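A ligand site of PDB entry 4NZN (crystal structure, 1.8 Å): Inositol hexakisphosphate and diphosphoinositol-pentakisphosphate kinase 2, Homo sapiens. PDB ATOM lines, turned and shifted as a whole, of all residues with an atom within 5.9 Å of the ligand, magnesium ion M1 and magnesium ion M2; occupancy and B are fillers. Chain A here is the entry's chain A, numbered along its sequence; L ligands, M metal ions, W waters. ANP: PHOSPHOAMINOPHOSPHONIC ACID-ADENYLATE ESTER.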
ATOM      1  N   ARG A  98      10.877  26.998  -7.979  1.00  0.00           N
ATOM      2  CA  ARG A  98       9.447  26.972  -8.269  1.00  0.00           C
ATOM      3  C   ARG A  98       9.119  27.382  -9.708  1.00  0.00           C
ATOM      4  O   ARG A  98       8.148  26.894 -10.290  1.00  0.00           O
ATOM      5  CB  ARG A  98       8.677  27.869  -7.312  1.00  0.00           C
ATOM      6  CG  ARG A  98       8.754  27.441  -5.865  1.00  0.00           C
ATOM      7  CD  ARG A  98       7.767  28.225  -5.008  1.00  0.00           C
ATOM      8  NE  ARG A  98       8.146  28.183  -3.603  1.00  0.00           N
ATOM      9  CZ  ARG A  98       7.721  27.288  -2.709  1.00  0.00           C
ATOM     10  NH1 ARG A  98       6.852  26.330  -3.040  1.00  0.00           N
ATOM     11  NH2 ARG A  98       8.168  27.347  -1.469  1.00  0.00           N
ATOM     12  N   TYR A 102       6.845  24.991 -12.146  1.00  0.00           N
ATOM     13  CA  TYR A 102       5.631  25.426 -12.816  1.00  0.00           C
ATOM     14  C   TYR A 102       5.750  25.370 -14.354  1.00  0.00           C
ATOM     15  O   TYR A 102       4.771  25.054 -15.021  1.00  0.00           O
ATOM     16  CB  TYR A 102       5.236  26.844 -12.360  1.00  0.00           C
ATOM     17  CG  TYR A 102       4.455  26.893 -11.058  1.00  0.00           C
ATOM     18  CD1 TYR A 102       4.539  25.869 -10.101  1.00  0.00           C
ATOM     19  CD2 TYR A 102       3.639  27.974 -10.794  1.00  0.00           C
ATOM     20  CE1 TYR A 102       3.799  25.930  -8.928  1.00  0.00           C
ATOM     21  CE2 TYR A 102       2.897  28.043  -9.626  1.00  0.00           C
ATOM     22  CZ  TYR A 102       2.976  27.039  -8.693  1.00  0.00           C
ATOM     23  OH  TYR A 102       2.238  27.143  -7.547  1.00  0.00           O
ATOM     24  N   PRO A 113      -2.487  26.891 -10.641  1.00  0.00           N
ATOM     25  CA  PRO A 113      -3.040  28.239 -10.484  1.00  0.00           C
ATOM     26  C   PRO A 113      -2.481  29.199 -11.526  1.00  0.00           C
ATOM     27  O   PRO A 113      -1.319  29.093 -11.912  1.00  0.00           O
ATOM     28  CB  PRO A 113      -2.601  28.642  -9.069  1.00  0.00           C
ATOM     29  CG  PRO A 113      -2.294  27.350  -8.364  1.00  0.00           C
ATOM     30  CD  PRO A 113      -1.782  26.434  -9.430  1.00  0.00           C
ATOM     31  N   VAL A 149      -1.545  34.557  -3.581  1.00  0.00           N
ATOM     32  CA  VAL A 149      -0.457  33.858  -2.900  1.00  0.00           C
ATOM     33  C   VAL A 149       0.890  34.321  -3.459  1.00  0.00           C
ATOM     34  O   VAL A 149       1.037  34.549  -4.681  1.00  0.00           O
ATOM     35  CB  VAL A 149      -0.619  32.331  -3.075  1.00  0.00           C
ATOM     36  CG1 VAL A 149       0.440  31.574  -2.285  1.00  0.00           C
ATOM     37  CG2 VAL A 149      -2.010  31.905  -2.655  1.00  0.00           C
ATOM     38  N   LYS A 151       4.911  33.277  -3.292  1.00  0.00           N
ATOM     39  CA  LYS A 151       5.849  32.212  -2.986  1.00  0.00           C
ATOM     40  C   LYS A 151       7.279  32.596  -3.371  1.00  0.00           C
ATOM     41  O   LYS A 151       7.519  33.049  -4.505  1.00  0.00           O
ATOM     42  CB  LYS A 151       5.463  30.926  -3.707  1.00  0.00           C
ATOM     43  CG  LYS A 151       4.043  30.456  -3.447  1.00  0.00           C
ATOM     44  CD  LYS A 151       3.808  29.094  -4.086  1.00  0.00           C
ATOM     45  CE  LYS A 151       2.410  28.623  -3.814  1.00  0.00           C
ATOM     46  NZ  LYS A 151       2.147  27.320  -4.465  1.00  0.00           N
ATOM     47  N   ALA A 155      12.079  26.868  -3.947  1.00  0.00           N
ATOM     48  CA  ALA A 155      11.153  25.873  -3.432  1.00  0.00           C
ATOM     49  C   ALA A 155      11.545  25.367  -2.033  1.00  0.00           C
ATOM     50  O   ALA A 155      10.738  24.760  -1.347  1.00  0.00           O
ATOM     51  CB  ALA A 155      11.043  24.713  -4.399  1.00  0.00           C
ATOM     52  N   ASP A 157      12.423  27.501   0.270  1.00  0.00           N
ATOM     53  CA  ASP A 157      12.025  28.583   1.185  1.00  0.00           C
ATOM     54  C   ASP A 157      10.508  28.489   1.372  1.00  0.00           C
ATOM     55  O   ASP A 157       9.742  28.723   0.436  1.00  0.00           O
ATOM     56  CB  ASP A 157      12.472  29.941   0.613  1.00  0.00           C
ATOM     57  CG  ASP A 157      12.089  31.141   1.501  1.00  0.00           C
ATOM     58  OD1 ASP A 157      11.237  31.018   2.408  1.00  0.00           O
ATOM     59  OD2 ASP A 157      12.651  32.229   1.267  1.00  0.00           O
ATOM     60  N   HIS A 158      10.100  28.110   2.580  1.00  0.00           N
ATOM     61  CA  HIS A 158       8.712  27.787   2.876  1.00  0.00           C
ATOM     62  C   HIS A 158       7.906  28.975   3.428  1.00  0.00           C
ATOM     63  O   HIS A 158       6.773  28.807   3.901  1.00  0.00           O
ATOM     64  CB  HIS A 158       8.670  26.581   3.828  1.00  0.00           C
ATOM     65  CG  HIS A 158       9.372  25.385   3.254  1.00  0.00           C
ATOM     66  ND1 HIS A 158       8.958  24.785   2.091  1.00  0.00           N
ATOM     67  CD2 HIS A 158      10.478  24.717   3.653  1.00  0.00           C
ATOM     68  CE1 HIS A 158       9.765  23.773   1.807  1.00  0.00           C
ATOM     69  NE2 HIS A 158      10.697  23.710   2.740  1.00  0.00           N
ATOM     70  N   ASN A 159       8.492  30.170   3.361  1.00  0.00           N
ATOM     71  CA  ASN A 159       7.812  31.403   3.756  1.00  0.00           C
ATOM     72  C   ASN A 159       6.855  31.891   2.652  1.00  0.00           C
ATOM     73  O   ASN A 159       7.109  32.891   1.978  1.00  0.00           O
ATOM     74  CB  ASN A 159       8.848  32.472   4.121  1.00  0.00           C
ATOM     75  CG  ASN A 159       9.691  32.042   5.316  1.00  0.00           C
ATOM     76  OD1 ASN A 159       9.174  31.886   6.417  1.00  0.00           O
ATOM     77  ND2 ASN A 159      10.970  31.810   5.095  1.00  0.00           N
ATOM     78  N   VAL A 160       5.755  31.163   2.492  1.00  0.00           N
ATOM     79  CA  VAL A 160       4.686  31.487   1.560  1.00  0.00           C
ATOM     80  C   VAL A 160       3.677  32.391   2.272  1.00  0.00           C
ATOM     81  O   VAL A 160       3.238  32.072   3.374  1.00  0.00           O
ATOM     82  CB  VAL A 160       3.993  30.199   1.102  1.00  0.00           C
ATOM     83  CG1 VAL A 160       2.744  30.468   0.291  1.00  0.00           C
ATOM     84  CG2 VAL A 160       4.972  29.346   0.289  1.00  0.00           C
ATOM     85  N   ILE A 162      -0.045  34.612   2.075  1.00  0.00           N
ATOM     86  CA  ILE A 162      -1.353  34.819   1.450  1.00  0.00           C
ATOM     87  C   ILE A 162      -1.864  36.206   1.851  1.00  0.00           C
ATOM     88  O   ILE A 162      -1.773  36.582   3.017  1.00  0.00           O
ATOM     89  CB  ILE A 162      -2.314  33.702   1.854  1.00  0.00           C
ATOM     90  CG1 ILE A 162      -1.682  32.342   1.461  1.00  0.00           C
ATOM     91  CG2 ILE A 162      -3.694  33.914   1.221  1.00  0.00           C
ATOM     92  CD1 ILE A 162      -2.551  31.148   1.752  1.00  0.00           C
ATOM     93  N   LEU A 175       2.924  31.707   6.165  1.00  0.00           N
ATOM     94  CA  LEU A 175       3.152  30.274   6.373  1.00  0.00           C
ATOM     95  C   LEU A 175       4.637  30.005   6.572  1.00  0.00           C
ATOM     96  O   LEU A 175       5.487  30.783   6.153  1.00  0.00           O
ATOM     97  CB  LEU A 175       2.613  29.460   5.189  1.00  0.00           C
ATOM     98  CG  LEU A 175       1.101  29.345   4.973  1.00  0.00           C
ATOM     99  CD1 LEU A 175       0.386  30.679   4.845  1.00  0.00           C
ATOM    100  CD2 LEU A 175       0.818  28.518   3.729  1.00  0.00           C
ATOM    101  N   GLU A 201       0.405  34.051  -7.430  1.00  0.00           N
ATOM    102  CA  GLU A 201      -0.625  33.198  -8.027  1.00  0.00           C
ATOM    103  C   GLU A 201      -2.005  33.376  -7.419  1.00  0.00           C
ATOM    104  O   GLU A 201      -2.159  33.831  -6.283  1.00  0.00           O
ATOM    105  CB  GLU A 201      -0.196  31.739  -7.997  1.00  0.00           C
ATOM    106  CG  GLU A 201       0.023  31.180  -6.633  1.00  0.00           C
ATOM    107  CD  GLU A 201       0.652  29.793  -6.643  1.00  0.00           C
ATOM    108  OE1 GLU A 201      -0.010  28.870  -6.148  1.00  0.00           O
ATOM    109  OE2 GLU A 201       1.786  29.636  -7.124  1.00  0.00           O
ATOM    110  N   GLU A 202      -3.010  33.018  -8.223  1.00  0.00           N
ATOM    111  CA  GLU A 202      -4.404  33.076  -7.787  1.00  0.00           C
ATOM    112  C   GLU A 202      -4.623  32.117  -6.632  1.00  0.00           C
ATOM    113  O   GLU A 202      -4.069  30.999  -6.627  1.00  0.00           O
ATOM    114  CB  GLU A 202      -5.383  32.772  -8.935  1.00  0.00           C
ATOM    115  CG  GLU A 202      -5.264  31.390  -9.521  1.00  0.00           C
ATOM    116  CD  GLU A 202      -6.398  30.987 -10.475  1.00  0.00           C
ATOM    117  OE1 GLU A 202      -7.557  31.448 -10.324  1.00  0.00           O
ATOM    118  OE2 GLU A 202      -6.112  30.161 -11.365  1.00  0.00           O
ATOM    119  N   PHE A 203      -5.398  32.559  -5.661  1.00  0.00           N
ATOM    120  CA  PHE A 203      -5.787  31.742  -4.534  1.00  0.00           C
ATOM    121  C   PHE A 203      -6.920  30.837  -4.971  1.00  0.00           C
ATOM    122  O   PHE A 203      -7.950  31.301  -5.473  1.00  0.00           O
ATOM    123  CB  PHE A 203      -6.227  32.612  -3.351  1.00  0.00           C
ATOM    124  CG  PHE A 203      -6.648  31.826  -2.145  1.00  0.00           C
ATOM    125  CD1 PHE A 203      -5.704  31.358  -1.255  1.00  0.00           C
ATOM    126  CD2 PHE A 203      -7.990  31.551  -1.919  1.00  0.00           C
ATOM    127  CE1 PHE A 203      -6.091  30.617  -0.140  1.00  0.00           C
ATOM    128  CE2 PHE A 203      -8.378  30.818  -0.810  1.00  0.00           C
ATOM    129  CZ  PHE A 203      -7.426  30.360   0.074  1.00  0.00           C
ATOM    130  N   MET A 204      -6.719  29.533  -4.795  1.00  0.00           N
ATOM    131  CA  MET A 204      -7.713  28.535  -5.174  1.00  0.00           C
ATOM    132  C   MET A 204      -8.523  28.141  -3.946  1.00  0.00           C
ATOM    133  O   MET A 204      -7.958  27.631  -2.973  1.00  0.00           O
ATOM    134  CB  MET A 204      -7.036  27.286  -5.747  1.00  0.00           C
ATOM    135  CG  MET A 204      -5.965  27.546  -6.806  1.00  0.00           C
ATOM    136  SD  MET A 204      -6.516  28.570  -8.186  1.00  0.00           S
ATOM    137  CE  MET A 204      -7.749  27.506  -8.929  1.00  0.00           C
ATOM    138  N   PRO A 205      -9.850  28.350  -4.001  1.00  0.00           N
ATOM    139  CA  PRO A 205     -10.702  28.048  -2.863  1.00  0.00           C
ATOM    140  C   PRO A 205     -10.944  26.544  -2.726  1.00  0.00           C
ATOM    141  O   PRO A 205     -11.510  25.933  -3.609  1.00  0.00           O
ATOM    142  CB  PRO A 205     -11.999  28.791  -3.199  1.00  0.00           C
ATOM    143  CG  PRO A 205     -12.052  28.793  -4.688  1.00  0.00           C
ATOM    144  CD  PRO A 205     -10.614  28.888  -5.141  1.00  0.00           C
ATOM    145  N   THR A 206     -10.487  25.974  -1.624  1.00  0.00           N
ATOM    146  CA  THR A 206     -10.702  24.560  -1.308  1.00  0.00           C
ATOM    147  C   THR A 206     -11.636  24.477  -0.100  1.00  0.00           C
ATOM    148  O   THR A 206     -12.074  25.509   0.436  1.00  0.00           O
ATOM    149  CB  THR A 206      -9.384  23.868  -0.936  1.00  0.00           C
ATOM    150  OG1 THR A 206      -8.898  24.379   0.313  1.00  0.00           O
ATOM    151  CG2 THR A 206      -8.333  24.088  -2.015  1.00  0.00           C
ATOM    152  N   ASP A 210      -5.606  20.407   2.063  1.00  0.00           N
ATOM    153  CA  ASP A 210      -4.682  20.148   0.976  1.00  0.00           C
ATOM    154  C   ASP A 210      -4.674  18.652   0.743  1.00  0.00           C
ATOM    155  O   ASP A 210      -4.695  17.889   1.711  1.00  0.00           O
ATOM    156  CB  ASP A 210      -3.232  20.452   1.385  1.00  0.00           C
ATOM    157  CG  ASP A 210      -2.990  21.887   1.694  1.00  0.00           C
ATOM    158  OD1 ASP A 210      -3.727  22.746   1.168  1.00  0.00           O
ATOM    159  OD2 ASP A 210      -2.014  22.147   2.444  1.00  0.00           O
ATOM    160  N   LYS A 212      -2.323  15.652  -0.361  1.00  0.00           N
ATOM    161  CA  LYS A 212      -0.917  15.297  -0.492  1.00  0.00           C
ATOM    162  C   LYS A 212      -0.835  13.970  -1.227  1.00  0.00           C
ATOM    163  O   LYS A 212      -1.427  12.982  -0.781  1.00  0.00           O
ATOM    164  CB  LYS A 212      -0.258  15.128   0.874  1.00  0.00           C
ATOM    165  CG  LYS A 212      -0.681  16.142   1.918  1.00  0.00           C
ATOM    166  CD  LYS A 212      -0.055  17.479   1.663  1.00  0.00           C
ATOM    167  CE  LYS A 212       1.353  17.537   2.244  1.00  0.00           C
ATOM    168  NZ  LYS A 212       1.949  18.880   1.988  1.00  0.00           N
ATOM    169  N   SER A 228      -5.259  22.819   5.656  1.00  0.00           N
ATOM    170  CA  SER A 228      -4.371  23.789   4.995  1.00  0.00           C
ATOM    171  C   SER A 228      -3.730  24.701   6.038  1.00  0.00           C
ATOM    172  O   SER A 228      -4.435  25.209   6.903  1.00  0.00           O
ATOM    173  CB  SER A 228      -5.144  24.660   4.015  1.00  0.00           C
ATOM    174  OG  SER A 228      -4.280  25.666   3.498  1.00  0.00           O
ATOM    175  N   PRO A 229      -2.432  24.916   5.960  1.00  0.00           N
ATOM    176  CA  PRO A 229      -1.753  25.857   6.862  1.00  0.00           C
ATOM    177  C   PRO A 229      -2.240  27.264   6.669  1.00  0.00           C
ATOM    178  O   PRO A 229      -2.089  28.101   7.504  1.00  0.00           O
ATOM    179  CB  PRO A 229      -0.271  25.724   6.490  1.00  0.00           C
ATOM    180  CG  PRO A 229      -0.166  24.504   5.709  1.00  0.00           C
ATOM    181  CD  PRO A 229      -1.472  24.314   5.038  1.00  0.00           C
ATOM    182  N   ALA A 230      -2.815  27.529   5.532  1.00  0.00           N
ATOM    183  CA  ALA A 230      -3.350  28.836   5.228  1.00  0.00           C
ATOM    184  C   ALA A 230      -4.572  29.162   6.049  1.00  0.00           C
ATOM    185  O   ALA A 230      -4.984  30.287   6.051  1.00  0.00           O
ATOM    186  CB  ALA A 230      -3.661  28.944   3.777  1.00  0.00           C
ATOM    187  N   ASP A 273       1.468  18.329  -4.104  1.00  0.00           N
ATOM    188  CA  ASP A 273       0.246  18.821  -3.459  1.00  0.00           C
ATOM    189  C   ASP A 273      -0.812  19.186  -4.500  1.00  0.00           C
ATOM    190  O   ASP A 273      -0.501  19.787  -5.532  1.00  0.00           O
ATOM    191  CB  ASP A 273       0.555  20.056  -2.603  1.00  0.00           C
ATOM    192  CG  ASP A 273       1.533  19.779  -1.492  1.00  0.00           C
ATOM    193  OD1 ASP A 273       1.449  18.692  -0.896  1.00  0.00           O
ATOM    194  OD2 ASP A 273       2.386  20.641  -1.194  1.00  0.00           O
ATOM    195  N   LEU A 275      -4.772  20.958  -4.952  1.00  0.00           N
ATOM    196  CA  LEU A 275      -5.833  21.790  -4.439  1.00  0.00           C
ATOM    197  C   LEU A 275      -7.099  21.411  -5.160  1.00  0.00           C
ATOM    198  O   LEU A 275      -7.182  21.604  -6.388  1.00  0.00           O
ATOM    199  CB  LEU A 275      -5.510  23.269  -4.662  1.00  0.00           C
ATOM    200  CG  LEU A 275      -4.167  23.705  -4.065  1.00  0.00           C
ATOM    201  CD1 LEU A 275      -3.839  25.150  -4.422  1.00  0.00           C
ATOM    202  CD2 LEU A 275      -4.162  23.491  -2.557  1.00  0.00           C
ATOM    203  N   CYS A 284      -0.033  22.620  -6.880  1.00  0.00           N
ATOM    204  CA  CYS A 284       0.594  23.866  -6.413  1.00  0.00           C
ATOM    205  C   CYS A 284       2.039  23.702  -5.934  1.00  0.00           C
ATOM    206  O   CYS A 284       2.685  24.686  -5.589  1.00  0.00           O
ATOM    207  CB  CYS A 284      -0.248  24.545  -5.325  1.00  0.00           C
ATOM    208  SG  CYS A 284      -0.319  23.652  -3.739  1.00  0.00           S
ATOM    209  N   ASP A 285       2.556  22.469  -5.912  1.00  0.00           N
ATOM    210  CA  ASP A 285       3.857  22.201  -5.307  1.00  0.00           C
ATOM    211  C   ASP A 285       4.268  20.793  -5.712  1.00  0.00           C
ATOM    212  O   ASP A 285       3.454  19.867  -5.641  1.00  0.00           O
ATOM    213  CB  ASP A 285       3.710  22.310  -3.788  1.00  0.00           C
ATOM    214  CG  ASP A 285       5.035  22.225  -3.029  1.00  0.00           C
ATOM    215  OD1 ASP A 285       6.122  22.567  -3.572  1.00  0.00           O
ATOM    216  OD2 ASP A 285       4.990  21.862  -1.825  1.00  0.00           O
ATOM    217  N   VAL A 286       5.507  20.635  -6.166  1.00  0.00           N
ATOM    218  CA  VAL A 286       6.112  19.329  -6.425  1.00  0.00           C
ATOM    219  C   VAL A 286       7.376  19.252  -5.595  1.00  0.00           C
ATOM    220  O   VAL A 286       8.278  20.081  -5.754  1.00  0.00           O
ATOM    221  CB  VAL A 286       6.456  19.141  -7.899  1.00  0.00           C
ATOM    222  CG1 VAL A 286       7.099  17.776  -8.148  1.00  0.00           C
ATOM    223  CG2 VAL A 286       5.200  19.311  -8.754  1.00  0.00           C
ATOM    224  N   ASN A 287       7.438  18.276  -4.689  1.00  0.00           N
ATOM    225  CA  ASN A 287       8.521  18.183  -3.714  1.00  0.00           C
ATOM    226  C   ASN A 287       9.584  17.131  -4.006  1.00  0.00           C
ATOM    227  O   ASN A 287      10.624  17.119  -3.351  1.00  0.00           O
ATOM    228  CB  ASN A 287       7.930  17.962  -2.330  1.00  0.00           C
ATOM    229  CG  ASN A 287       7.123  19.152  -1.850  1.00  0.00           C
ATOM    230  OD1 ASN A 287       7.529  20.301  -2.074  1.00  0.00           O
ATOM    231  ND2 ASN A 287       5.966  18.907  -1.244  1.00  0.00           N
HETATM  232  PG  ANP L   1       5.985  21.880   1.290  1.00  0.00           P
HETATM  233  O1G ANP L   1       4.815  21.020   0.840  1.00  0.00           O
HETATM  234  O2G ANP L   1       6.317  21.694   2.765  1.00  0.00           O
HETATM  235  O3G ANP L   1       7.212  21.781   0.373  1.00  0.00           O
HETATM  236  PB  ANP L   1       5.839  24.742   0.212  1.00  0.00           P
HETATM  237  O1B ANP L   1       6.481  24.124  -1.028  1.00  0.00           O
HETATM  238  O2B ANP L   1       6.679  25.738   0.924  1.00  0.00           O
HETATM  239  N3B ANP L   1       5.274  23.476   1.222  1.00  0.00           N
HETATM  240  PA  ANP L   1       3.248  25.198  -1.054  1.00  0.00           P
HETATM  241  O1A ANP L   1       3.292  25.677  -2.473  1.00  0.00           O
HETATM  242  O2A ANP L   1       2.900  23.767  -0.764  1.00  0.00           O
HETATM  243  O3A ANP L   1       4.590  25.618  -0.270  1.00  0.00           O
HETATM  244  O5' ANP L   1       2.192  26.151  -0.287  1.00  0.00           O
HETATM  245  C5' ANP L   1       1.906  25.895   1.084  1.00  0.00           C
HETATM  246  C4' ANP L   1       0.419  25.752   1.298  1.00  0.00           C
HETATM  247  O4' ANP L   1      -0.209  26.980   0.933  1.00  0.00           O
HETATM  248  C3' ANP L   1      -0.269  24.685   0.463  1.00  0.00           C
HETATM  249  O3' ANP L   1      -0.155  23.373   1.019  1.00  0.00           O
HETATM  250  C2' ANP L   1      -1.688  25.203   0.398  1.00  0.00           C
HETATM  251  O2' ANP L   1      -2.464  24.923   1.587  1.00  0.00           O
HETATM  252  C1' ANP L   1      -1.469  26.695   0.306  1.00  0.00           C
HETATM  253  N9  ANP L   1      -1.400  27.176  -1.080  1.00  0.00           N
HETATM  254  C8  ANP L   1      -0.309  27.269  -1.894  1.00  0.00           C
HETATM  255  N7  ANP L   1      -0.655  27.792  -3.106  1.00  0.00           N
HETATM  256  C5  ANP L   1      -1.968  28.025  -3.048  1.00  0.00           C
HETATM  257  C6  ANP L   1      -2.967  28.578  -3.975  1.00  0.00           C
HETATM  258  N6  ANP L   1      -2.572  28.967  -5.201  1.00  0.00           N
HETATM  259  N1  ANP L   1      -4.245  28.688  -3.547  1.00  0.00           N
HETATM  260  C2  ANP L   1      -4.617  28.284  -2.314  1.00  0.00           C
HETATM  261  N3  ANP L   1      -3.749  27.768  -1.422  1.00  0.00           N
HETATM  262  C4  ANP L   1      -2.451  27.629  -1.728  1.00  0.00           C
HETATM  263 MG    MG M   1       7.213  22.229  -1.508  1.00  0.00          MG
HETATM  264 MG    MG M   2       3.517  21.966  -0.286  1.00  0.00          MG
HETATM  265  O   HOH W   1       3.234  22.767   3.639  1.00  0.00           O
HETATM  266  O   HOH W   2       4.961  26.988   2.935  1.00  0.00           O
HETATM  267  O   HOH W   3       2.101  21.980   1.304  1.00  0.00           O
HETATM  268  O   HOH W   4       8.513  22.049   4.928  1.00  0.00           O
HETATM  269  O   HOH W   5       4.558  20.456   4.876  1.00  0.00           O
HETATM  270  O   HOH W   6       8.872  22.718  -2.062  1.00  0.00           O
HETATM  271  O   HOH W   7       3.306  25.302   4.206  1.00  0.00           O
HETATM  272  O   HOH W   8      -5.511  26.810   0.643  1.00  0.00           O
HETATM  273  O   HOH W   9       4.460  18.959   2.427  1.00  0.00           O
HETATM  274  O   HOH W  10       6.186  23.960   4.773  1.00  0.00           O
HETATM  275  O   HOH W  11       9.361  19.937   0.536  1.00  0.00           O
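The side-chain carboxylate (OD1) of Asp 273 lies within salt-bridge range of the side-chain amino group (NZ) of Lys 212 (2.9 Å).
NH1 of Arg 98 sits close to OD1 of Asp 285, at 3.9 Å.
The backbone carbonyl oxygen of Glu 201 is in hydrogen-bond range of the backbone NH of Val 149.
OE2 of Glu 201 sits at hydrogen-bond distance from OH of Tyr 102 (2.6 Å).
The side-chain hydroxyl (OG) of Ser 228 sits close to the backbone NH (N) of Ala 230.
NZ of Lys 151 sits at hydrogen-bond distance from O of Cys 284 (2.9 Å).
O of Cys 284 lies within hydrogen-bond range of OH of Tyr 102 (3.2 Å).
The backbone NH of Leu 175 lies within hydrogen-bond range of the backbone carbonyl oxygen of Val 160 (2.8 Å).
The side-chain carboxylate of Asp 210 lies within hydrogen-bond range of an oxygen (O2') of the ligand, 2.6 Å away.
An oxygen (O2B) of the ligand is in hydrogen-bond range of a ring nitrogen (ND1) of His 158 (2.7 Å).
OE1 of Glu 201 lies within hydrogen-bond range of N6 of the ligand (2.7 Å).
O2' of the ligand lies within hydrogen-bond range of OG of Ser 228, at 2.7 Å.
The side-chain amino group (NZ) of Lys 151 is in salt-bridge range of an oxygen (O1A) of the ligand, at 2.8 Å.
The backbone NH (N) of Met 204 is in hydrogen-bond range of a nitrogen (N1) of the ligand.
The backbone carbonyl oxygen (O) of Glu 202 sits at hydrogen-bond distance from a nitrogen (N6) of the ligand (2.9 Å).
The guanidinium group (NH2) of Arg 98 lies within salt-bridge range of an oxygen (O2B) of the ligand.
An oxygen (O1G) of the ligand lies close to the side-chain amino group of Lys 212 (3.8 Å).
Magnesium ion M1 is bound by water W6 (1.8 Å), O3G of the ligand (1.9 Å), OD1 of Asn 287 (2.0 Å), O1B of the ligand (2.1 Å), OD2 of Asp 285 (2.3 Å) and OD1 of Asp 285 (2.4 Å).
Magnesium ion M1 has six donor atoms within binding distance.
Water W3 lies within hydrogen-bond range of O3' of the ligand (2.7 Å) and NZ of Lys 212 (3.2 Å).
Water W9 bridges NZ of Lys 212 (2.6 Å) and O2G of the ligand (3.3 Å).
Water W8 bridges a nitrogen (N3) of the ligand (2.9 Å) and the side-chain hydroxyl of Ser 228 (3.3 Å).
Water W2 lies within hydrogen-bond range of the backbone carbonyl oxygen of His 158 (2.7 Å) and an oxygen (O2B) of the ligand (2.9 Å).
O of Cys 284 lies close to O1A of the ligand, at 3.3 Å.
Merely in contact with the ligand: Leu 175, Phe 203, Pro 113, Leu 275, Pro 229, Val 149 and Val 160.
Hydrophobic or aromatic side chains within 4 Å of the ligand: Pro 113, Val 149, His 158, Val 160, Leu 175, Phe 203, Met 204, Pro 229 and Leu 275.
Within 4 Å of the ligand: Arg 98, Pro 113, Val 149, Lys 151, His 158, Val 160, Leu 175, Glu 201, Glu 202, Phe 203, Met 204, Asp 210, Lys 212, Ser 228, Pro 229, Asp 273, Leu 275, Cys 284, Asp 285 and Asn 287.
The nearest printed residue that does not touch the ligand is Asp 157 (4.3 Å).
Of the 29 residues printed, 2 come within 4 Å of magnesium ion M2.
Along chain A the residues within 4 Å of magnesium ion M2 span positions 273 to 285.
Magnesium ion M2 is bound by an oxygen (O1G) of the ligand (2.0 Å), the side-chain carboxylate of Asp 273 (2.0 Å), an oxygen (O2A) of the ligand (2.0 Å), water W3 (2.1 Å) and the side-chain carboxylate of Asp 285 (2.1 Å).
Slightly farther from magnesium ion M2 lies a nitrogen (N3B) of the ligand (2.8 Å).
Within 4 Å of magnesium ion M1: Asp 285 and Asn 287.
Along chain A the residues within 4 Å of magnesium ion M1 span positions 285 to 287.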
